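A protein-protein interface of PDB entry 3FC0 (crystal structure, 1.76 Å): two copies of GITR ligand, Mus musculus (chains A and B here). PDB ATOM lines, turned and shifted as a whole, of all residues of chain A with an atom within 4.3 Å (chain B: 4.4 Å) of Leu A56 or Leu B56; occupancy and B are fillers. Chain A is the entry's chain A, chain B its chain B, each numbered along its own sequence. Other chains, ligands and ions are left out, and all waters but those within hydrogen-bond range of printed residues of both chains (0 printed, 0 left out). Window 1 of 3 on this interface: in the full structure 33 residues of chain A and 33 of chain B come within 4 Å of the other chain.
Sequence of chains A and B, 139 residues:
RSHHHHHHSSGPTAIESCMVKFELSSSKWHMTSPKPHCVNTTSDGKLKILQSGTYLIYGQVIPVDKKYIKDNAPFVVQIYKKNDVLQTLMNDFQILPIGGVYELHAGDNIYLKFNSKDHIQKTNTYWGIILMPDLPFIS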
ATOM      1  N   TYR A  55     -12.848 -19.870 -17.045  1.00  0.00           N
ATOM      2  CA  TYR A  55     -12.591 -21.047 -17.857  1.00  0.00           C
ATOM      3  C   TYR A  55     -12.259 -20.704 -19.277  1.00  0.00           C
ATOM      4  O   TYR A  55     -12.740 -19.708 -19.802  1.00  0.00           O
ATOM      5  CB  TYR A  55     -13.823 -21.947 -17.902  1.00  0.00           C
ATOM      6  CG  TYR A  55     -14.143 -22.638 -16.615  1.00  0.00           C
ATOM      7  CD1 TYR A  55     -14.835 -21.972 -15.616  1.00  0.00           C
ATOM      8  CD2 TYR A  55     -13.779 -23.962 -16.426  1.00  0.00           C
ATOM      9  CE1 TYR A  55     -15.167 -22.623 -14.404  1.00  0.00           C
ATOM     10  CE2 TYR A  55     -14.099 -24.617 -15.228  1.00  0.00           C
ATOM     11  CZ  TYR A  55     -14.761 -23.930 -14.233  1.00  0.00           C
ATOM     12  OH  TYR A  55     -15.119 -24.605 -13.092  1.00  0.00           O
ATOM     13  N   LEU A  56     -11.457 -21.547 -19.900  1.00  0.00           N
ATOM     14  CA  LEU A  56     -11.253 -21.493 -21.351  1.00  0.00           C
ATOM     15  C   LEU A  56     -12.090 -22.628 -21.966  1.00  0.00           C
ATOM     16  O   LEU A  56     -11.828 -23.810 -21.700  1.00  0.00           O
ATOM     17  CB  LEU A  56      -9.800 -21.701 -21.700  1.00  0.00           C
ATOM     18  CG  LEU A  56      -9.396 -21.822 -23.188  1.00  0.00           C
ATOM     19  CD1 LEU A  56      -9.862 -20.589 -23.977  1.00  0.00           C
ATOM     20  CD2 LEU A  56      -7.911 -21.981 -23.327  1.00  0.00           C
ATOM     21  N   ILE A  57     -13.125 -22.256 -22.715  1.00  0.00           N
ATOM     22  CA  ILE A  57     -13.933 -23.230 -23.454  1.00  0.00           C
ATOM     23  C   ILE A  57     -13.262 -23.350 -24.820  1.00  0.00           C
ATOM     24  O   ILE A  57     -12.837 -22.336 -25.403  1.00  0.00           O
ATOM     25  CB  ILE A  57     -15.361 -22.707 -23.667  1.00  0.00           C
ATOM     26  CG1 ILE A  57     -16.050 -22.474 -22.313  1.00  0.00           C
ATOM     27  CG2 ILE A  57     -16.136 -23.669 -24.594  1.00  0.00           C
ATOM     28  CD1 ILE A  57     -17.410 -21.743 -22.410  1.00  0.00           C
ATOM     29  N   TYR A  58     -13.082 -24.562 -25.315  1.00  0.00           N
ATOM     30  CA  TYR A  58     -12.332 -24.725 -26.552  1.00  0.00           C
ATOM     31  C   TYR A  58     -12.928 -25.847 -27.386  1.00  0.00           C
ATOM     32  O   TYR A  58     -13.819 -26.590 -26.931  1.00  0.00           O
ATOM     33  CB  TYR A  58     -10.814 -25.004 -26.300  1.00  0.00           C
ATOM     34  CG  TYR A  58     -10.627 -26.335 -25.643  1.00  0.00           C
ATOM     35  CD1 TYR A  58     -10.291 -27.440 -26.394  1.00  0.00           C
ATOM     36  CD2 TYR A  58     -10.892 -26.514 -24.269  1.00  0.00           C
ATOM     37  CE1 TYR A  58     -10.162 -28.667 -25.813  1.00  0.00           C
ATOM     38  CE2 TYR A  58     -10.735 -27.776 -23.660  1.00  0.00           C
ATOM     39  CZ  TYR A  58     -10.409 -28.845 -24.473  1.00  0.00           C
ATOM     40  OH  TYR A  58     -10.274 -30.138 -23.997  1.00  0.00           O
ATOM     41  N   GLY A 100     -13.340 -19.606 -26.093  1.00  0.00           N
ATOM     42  CA  GLY A 100     -12.786 -18.354 -25.555  1.00  0.00           C
ATOM     43  C   GLY A 100     -12.728 -18.452 -24.049  1.00  0.00           C
ATOM     44  O   GLY A 100     -13.123 -19.467 -23.458  1.00  0.00           O
ATOM     45  N   VAL A 101     -12.272 -17.358 -23.435  1.00  0.00           N
ATOM     46  CA  VAL A 101     -12.254 -17.215 -21.967  1.00  0.00           C
ATOM     47  C   VAL A 101     -13.594 -16.639 -21.463  1.00  0.00           C
ATOM     48  O   VAL A 101     -14.042 -15.580 -21.914  1.00  0.00           O
ATOM     49  CB  VAL A 101     -11.125 -16.240 -21.568  1.00  0.00           C
ATOM     50  CG1 VAL A 101     -11.195 -15.976 -20.038  1.00  0.00           C
ATOM     51  CG2 VAL A 101      -9.775 -16.784 -22.028  1.00  0.00           C
ATOM     52  N   GLY A 128     -14.336 -28.853 -25.166  1.00  0.00           N
ATOM     53  CA  GLY A 128     -14.071 -29.153 -23.741  1.00  0.00           C
ATOM     54  C   GLY A 128     -13.832 -27.851 -23.008  1.00  0.00           C
ATOM     55  O   GLY A 128     -14.109 -26.784 -23.555  1.00  0.00           O
ATOM     56  N   ILE A 129     -13.401 -27.941 -21.737  1.00  0.00           N
ATOM     57  CA  ILE A 129     -13.145 -26.741 -20.966  1.00  0.00           C
ATOM     58  C   ILE A 129     -11.933 -27.000 -20.110  1.00  0.00           C
ATOM     59  O   ILE A 129     -11.574 -28.160 -19.857  1.00  0.00           O
ATOM     60  CB  ILE A 129     -14.274 -26.303 -20.042  1.00  0.00           C
ATOM     61  CG1 ILE A 129     -14.556 -27.345 -18.954  1.00  0.00           C
ATOM     62  CG2 ILE A 129     -15.572 -26.043 -20.779  1.00  0.00           C
ATOM     63  CD1 ILE A 129     -15.481 -26.843 -17.926  1.00  0.00           C
ATOM     64  N   ILE A 130     -11.281 -25.924 -19.711  1.00  0.00           N
ATOM     65  CA  ILE A 130     -10.147 -26.003 -18.778  1.00  0.00           C
ATOM     66  C   ILE A 130     -10.351 -24.862 -17.757  1.00  0.00           C
ATOM     67  O   ILE A 130     -10.596 -23.715 -18.111  1.00  0.00           O
ATOM     68  CB  ILE A 130      -8.777 -25.928 -19.485  1.00  0.00           C
ATOM     69  CG1 ILE A 130      -7.626 -25.889 -18.405  1.00  0.00           C
ATOM     70  CG2 ILE A 130      -8.752 -24.713 -20.337  1.00  0.00           C
ATOM     71  CD1 ILE A 130      -6.240 -26.250 -18.911  1.00  0.00           C
ATOM     72  N   MET A 132      -8.962 -22.180 -15.602  1.00  0.00           N
ATOM     73  CA  MET A 132      -7.752 -21.438 -15.853  1.00  0.00           C
ATOM     74  C   MET A 132      -7.037 -21.051 -14.550  1.00  0.00           C
ATOM     75  O   MET A 132      -7.684 -20.765 -13.584  1.00  0.00           O
ATOM     76  CB  MET A 132      -8.078 -20.161 -16.635  1.00  0.00           C
ATOM     77  CG  MET A 132      -8.166 -20.429 -18.153  1.00  0.00           C
ATOM     78  SD  MET A 132      -8.954 -18.983 -18.939  1.00  0.00           S
ATOM     79  CE  MET A 132      -7.884 -17.638 -18.385  1.00  0.00           C
ATOM     80  N   TYR B  55      -0.101 -28.361 -26.474  1.00  0.00           N
ATOM     81  CA  TYR B  55      -0.592 -27.043 -26.126  1.00  0.00           C
ATOM     82  C   TYR B  55      -1.992 -26.786 -26.637  1.00  0.00           C
ATOM     83  O   TYR B  55      -2.377 -27.311 -27.685  1.00  0.00           O
ATOM     84  CB  TYR B  55       0.310 -25.988 -26.726  1.00  0.00           C
ATOM     85  CG  TYR B  55       1.644 -25.895 -25.998  1.00  0.00           C
ATOM     86  CD1 TYR B  55       1.827 -24.966 -24.968  1.00  0.00           C
ATOM     87  CD2 TYR B  55       2.695 -26.724 -26.347  1.00  0.00           C
ATOM     88  CE1 TYR B  55       3.077 -24.895 -24.289  1.00  0.00           C
ATOM     89  CE2 TYR B  55       3.940 -26.655 -25.682  1.00  0.00           C
ATOM     90  CZ  TYR B  55       4.107 -25.731 -24.668  1.00  0.00           C
ATOM     91  OH  TYR B  55       5.335 -25.648 -24.012  1.00  0.00           O
ATOM     92  N   LEU B  56      -2.739 -25.994 -25.874  1.00  0.00           N
ATOM     93  CA  LEU B  56      -3.971 -25.368 -26.415  1.00  0.00           C
ATOM     94  C   LEU B  56      -3.658 -23.944 -26.841  1.00  0.00           C
ATOM     95  O   LEU B  56      -3.324 -23.080 -25.992  1.00  0.00           O
ATOM     96  CB  LEU B  56      -5.082 -25.420 -25.394  1.00  0.00           C
ATOM     97  CG  LEU B  56      -6.427 -24.743 -25.703  1.00  0.00           C
ATOM     98  CD1 LEU B  56      -6.975 -25.226 -27.058  1.00  0.00           C
ATOM     99  CD2 LEU B  56      -7.340 -25.112 -24.569  1.00  0.00           C
ATOM    100  N   ILE B  57      -3.710 -23.704 -28.155  1.00  0.00           N
ATOM    101  CA  ILE B  57      -3.570 -22.349 -28.684  1.00  0.00           C
ATOM    102  C   ILE B  57      -4.990 -21.789 -28.734  1.00  0.00           C
ATOM    103  O   ILE B  57      -5.906 -22.512 -29.150  1.00  0.00           O
ATOM    104  CB  ILE B  57      -2.994 -22.359 -30.089  1.00  0.00           C
ATOM    105  CG1 ILE B  57      -1.615 -23.043 -30.141  1.00  0.00           C
ATOM    106  CG2 ILE B  57      -2.951 -20.959 -30.626  1.00  0.00           C
ATOM    107  CD1 ILE B  57      -1.031 -23.028 -31.515  1.00  0.00           C
ATOM    108  N   TYR B  58      -5.217 -20.548 -28.273  1.00  0.00           N
ATOM    109  CA  TYR B  58      -6.584 -20.014 -28.160  1.00  0.00           C
ATOM    110  C   TYR B  58      -6.627 -18.514 -28.404  1.00  0.00           C
ATOM    111  O   TYR B  58      -5.589 -17.845 -28.480  1.00  0.00           O
ATOM    112  CB  TYR B  58      -7.213 -20.306 -26.771  1.00  0.00           C
ATOM    113  CG  TYR B  58      -6.549 -19.479 -25.703  1.00  0.00           C
ATOM    114  CD1 TYR B  58      -7.123 -18.291 -25.297  1.00  0.00           C
ATOM    115  CD2 TYR B  58      -5.328 -19.867 -25.162  1.00  0.00           C
ATOM    116  CE1 TYR B  58      -6.497 -17.476 -24.330  1.00  0.00           C
ATOM    117  CE2 TYR B  58      -4.670 -19.056 -24.212  1.00  0.00           C
ATOM    118  CZ  TYR B  58      -5.261 -17.881 -23.818  1.00  0.00           C
ATOM    119  OH  TYR B  58      -4.644 -17.045 -22.890  1.00  0.00           O
ATOM    120  N   GLY B 100      -6.787 -24.408 -31.111  1.00  0.00           N
ATOM    121  CA  GLY B 100      -7.093 -25.794 -30.950  1.00  0.00           C
ATOM    122  C   GLY B 100      -5.926 -26.469 -30.236  1.00  0.00           C
ATOM    123  O   GLY B 100      -4.978 -25.791 -29.789  1.00  0.00           O
ATOM    124  N   VAL B 101      -6.008 -27.776 -30.112  1.00  0.00           N
ATOM    125  CA  VAL B 101      -4.902 -28.566 -29.511  1.00  0.00           C
ATOM    126  C   VAL B 101      -3.815 -28.939 -30.526  1.00  0.00           C
ATOM    127  O   VAL B 101      -4.090 -29.561 -31.601  1.00  0.00           O
ATOM    128  CB  VAL B 101      -5.467 -29.820 -28.846  1.00  0.00           C
ATOM    129  CG1 VAL B 101      -4.289 -30.686 -28.243  1.00  0.00           C
ATOM    130  CG2 VAL B 101      -6.573 -29.474 -27.828  1.00  0.00           C
ATOM    131  N   GLY B 128      -3.369 -16.579 -27.028  1.00  0.00           N
ATOM    132  CA  GLY B 128      -2.395 -17.106 -26.076  1.00  0.00           C
ATOM    133  C   GLY B 128      -2.219 -18.582 -26.224  1.00  0.00           C
ATOM    134  O   GLY B 128      -2.722 -19.162 -27.165  1.00  0.00           O
ATOM    135  N   ILE B 129      -1.505 -19.190 -25.275  1.00  0.00           N
ATOM    136  CA  ILE B 129      -1.358 -20.608 -25.229  1.00  0.00           C
ATOM    137  C   ILE B 129      -1.376 -21.061 -23.778  1.00  0.00           C
ATOM    138  O   ILE B 129      -1.136 -20.260 -22.839  1.00  0.00           O
ATOM    139  CB  ILE B 129      -0.043 -21.119 -25.802  1.00  0.00           C
ATOM    140  CG1 ILE B 129       1.131 -20.581 -24.992  1.00  0.00           C
ATOM    141  CG2 ILE B 129       0.143 -20.794 -27.240  1.00  0.00           C
ATOM    142  CD1 ILE B 129       2.380 -21.260 -25.415  1.00  0.00           C
ATOM    143  N   ILE B 130      -1.709 -22.330 -23.610  1.00  0.00           N
ATOM    144  CA  ILE B 130      -1.627 -23.041 -22.315  1.00  0.00           C
ATOM    145  C   ILE B 130      -1.009 -24.432 -22.537  1.00  0.00           C
ATOM    146  O   ILE B 130      -1.391 -25.189 -23.441  1.00  0.00           O
ATOM    147  CB  ILE B 130      -2.988 -23.021 -21.491  1.00  0.00           C
ATOM    148  CG1 ILE B 130      -2.812 -23.792 -20.157  1.00  0.00           C
ATOM    149  CG2 ILE B 130      -4.113 -23.628 -22.272  1.00  0.00           C
ATOM    150  CD1 ILE B 130      -3.910 -23.642 -19.133  1.00  0.00           C
ATOM    151  N   MET B 132      -0.822 -28.078 -21.829  1.00  0.00           N
ATOM    152  CA  MET B 132      -1.874 -28.911 -21.284  1.00  0.00           C
ATOM    153  C   MET B 132      -1.334 -30.017 -20.357  1.00  0.00           C
ATOM    154  O   MET B 132      -0.300 -30.589 -20.644  1.00  0.00           O
ATOM    155  CB  MET B 132      -2.708 -29.550 -22.392  1.00  0.00           C
ATOM    156  CG  MET B 132      -3.746 -28.568 -23.048  1.00  0.00           C
ATOM    157  SD  MET B 132      -4.186 -29.187 -24.711  1.00  0.00           S
ATOM    158  CE  MET B 132      -4.664 -30.866 -24.335  1.00  0.00           C
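The backbone carbonyl oxygen of Tyr A58 lies within hydrogen-bond range of the backbone NH of Gly A128 (2.9 Å).
The backbone carbonyl oxygen (O) of Tyr B58 sits at hydrogen-bond distance from the backbone NH (N) of Gly B128 (2.9 Å).
N of Leu A56 is in hydrogen-bond range of SD of Met A132 (3.7 Å).
The side-chain sulfur (SD) of Met B132 lies within hydrogen-bond range of the backbone NH (N) of Leu B56, 3.7 Å away.
The backbone NH (N) of Leu A56 is in hydrogen-bond range of the backbone carbonyl oxygen (O) of Ile A130 (2.9 Å).
The backbone carbonyl oxygen (O) of Ile B130 lies within hydrogen-bond range of the backbone NH (N) of Leu B56, at 2.9 Å.
CD2 of Leu A56 touches CD2 of Leu B56, 3.4 Å away.
Leu A56 touches Tyr B58 (CD2 to CG, 3.7 Å).
Leu B56 touches Tyr A58 (CD2 to CG, 3.7 Å).
Ile A130 touches Ile B130.
Of chain B, only Leu B56 (3.4 Å) and Tyr B58 (3.7 Å) come within 4 Å of Leu A56.
Of the printed residues of chain B, Tyr A58 touches Leu B56 (3.7 Å).
Printed residues of chain B within 4 Å of Ile A130: Ile B130.
Of the printed residues of chain A, Tyr B58 touches Leu A56 (3.7 Å).
Of the printed residues of chain A, Ile B130 touches Ile A130.
The nearest printed residue of chain A that does not touch Leu B56 is Ile A130 (4.5 Å).
The nearest printed residue of chain B that does not touch Tyr A58 is Val B101 (4.2 Å).
Of the 10 printed residues of chain B, 3 touch a printed residue of chain A.
Printed residues of chain B that touch a printed residue of chain A: Leu B56, Tyr B58 and Ile B130.
Along chain B the printed residues that touch a printed residue of chain A span positions 56 to 130.
Of the 10 printed residues of chain A, 3 touch a printed residue of chain B.
Hydrophobic or aromatic side chains of chain A that line the printed part of chain B: Leu A56, Tyr A58 and Ile A130.
Among the printed residues, no Asp or Glu carboxylate lies within 4 Å of a Lys or Arg side-chain nitrogen of the other chain.
Leu B56 touches its own counterpart, Leu A56.
Leu A56 touches Tyr B58, and with the chains exchanged Tyr A58 touches Leu B56.
Ile B130 touches its own counterpart, Ile A130.
10 positions are printed for both chains.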
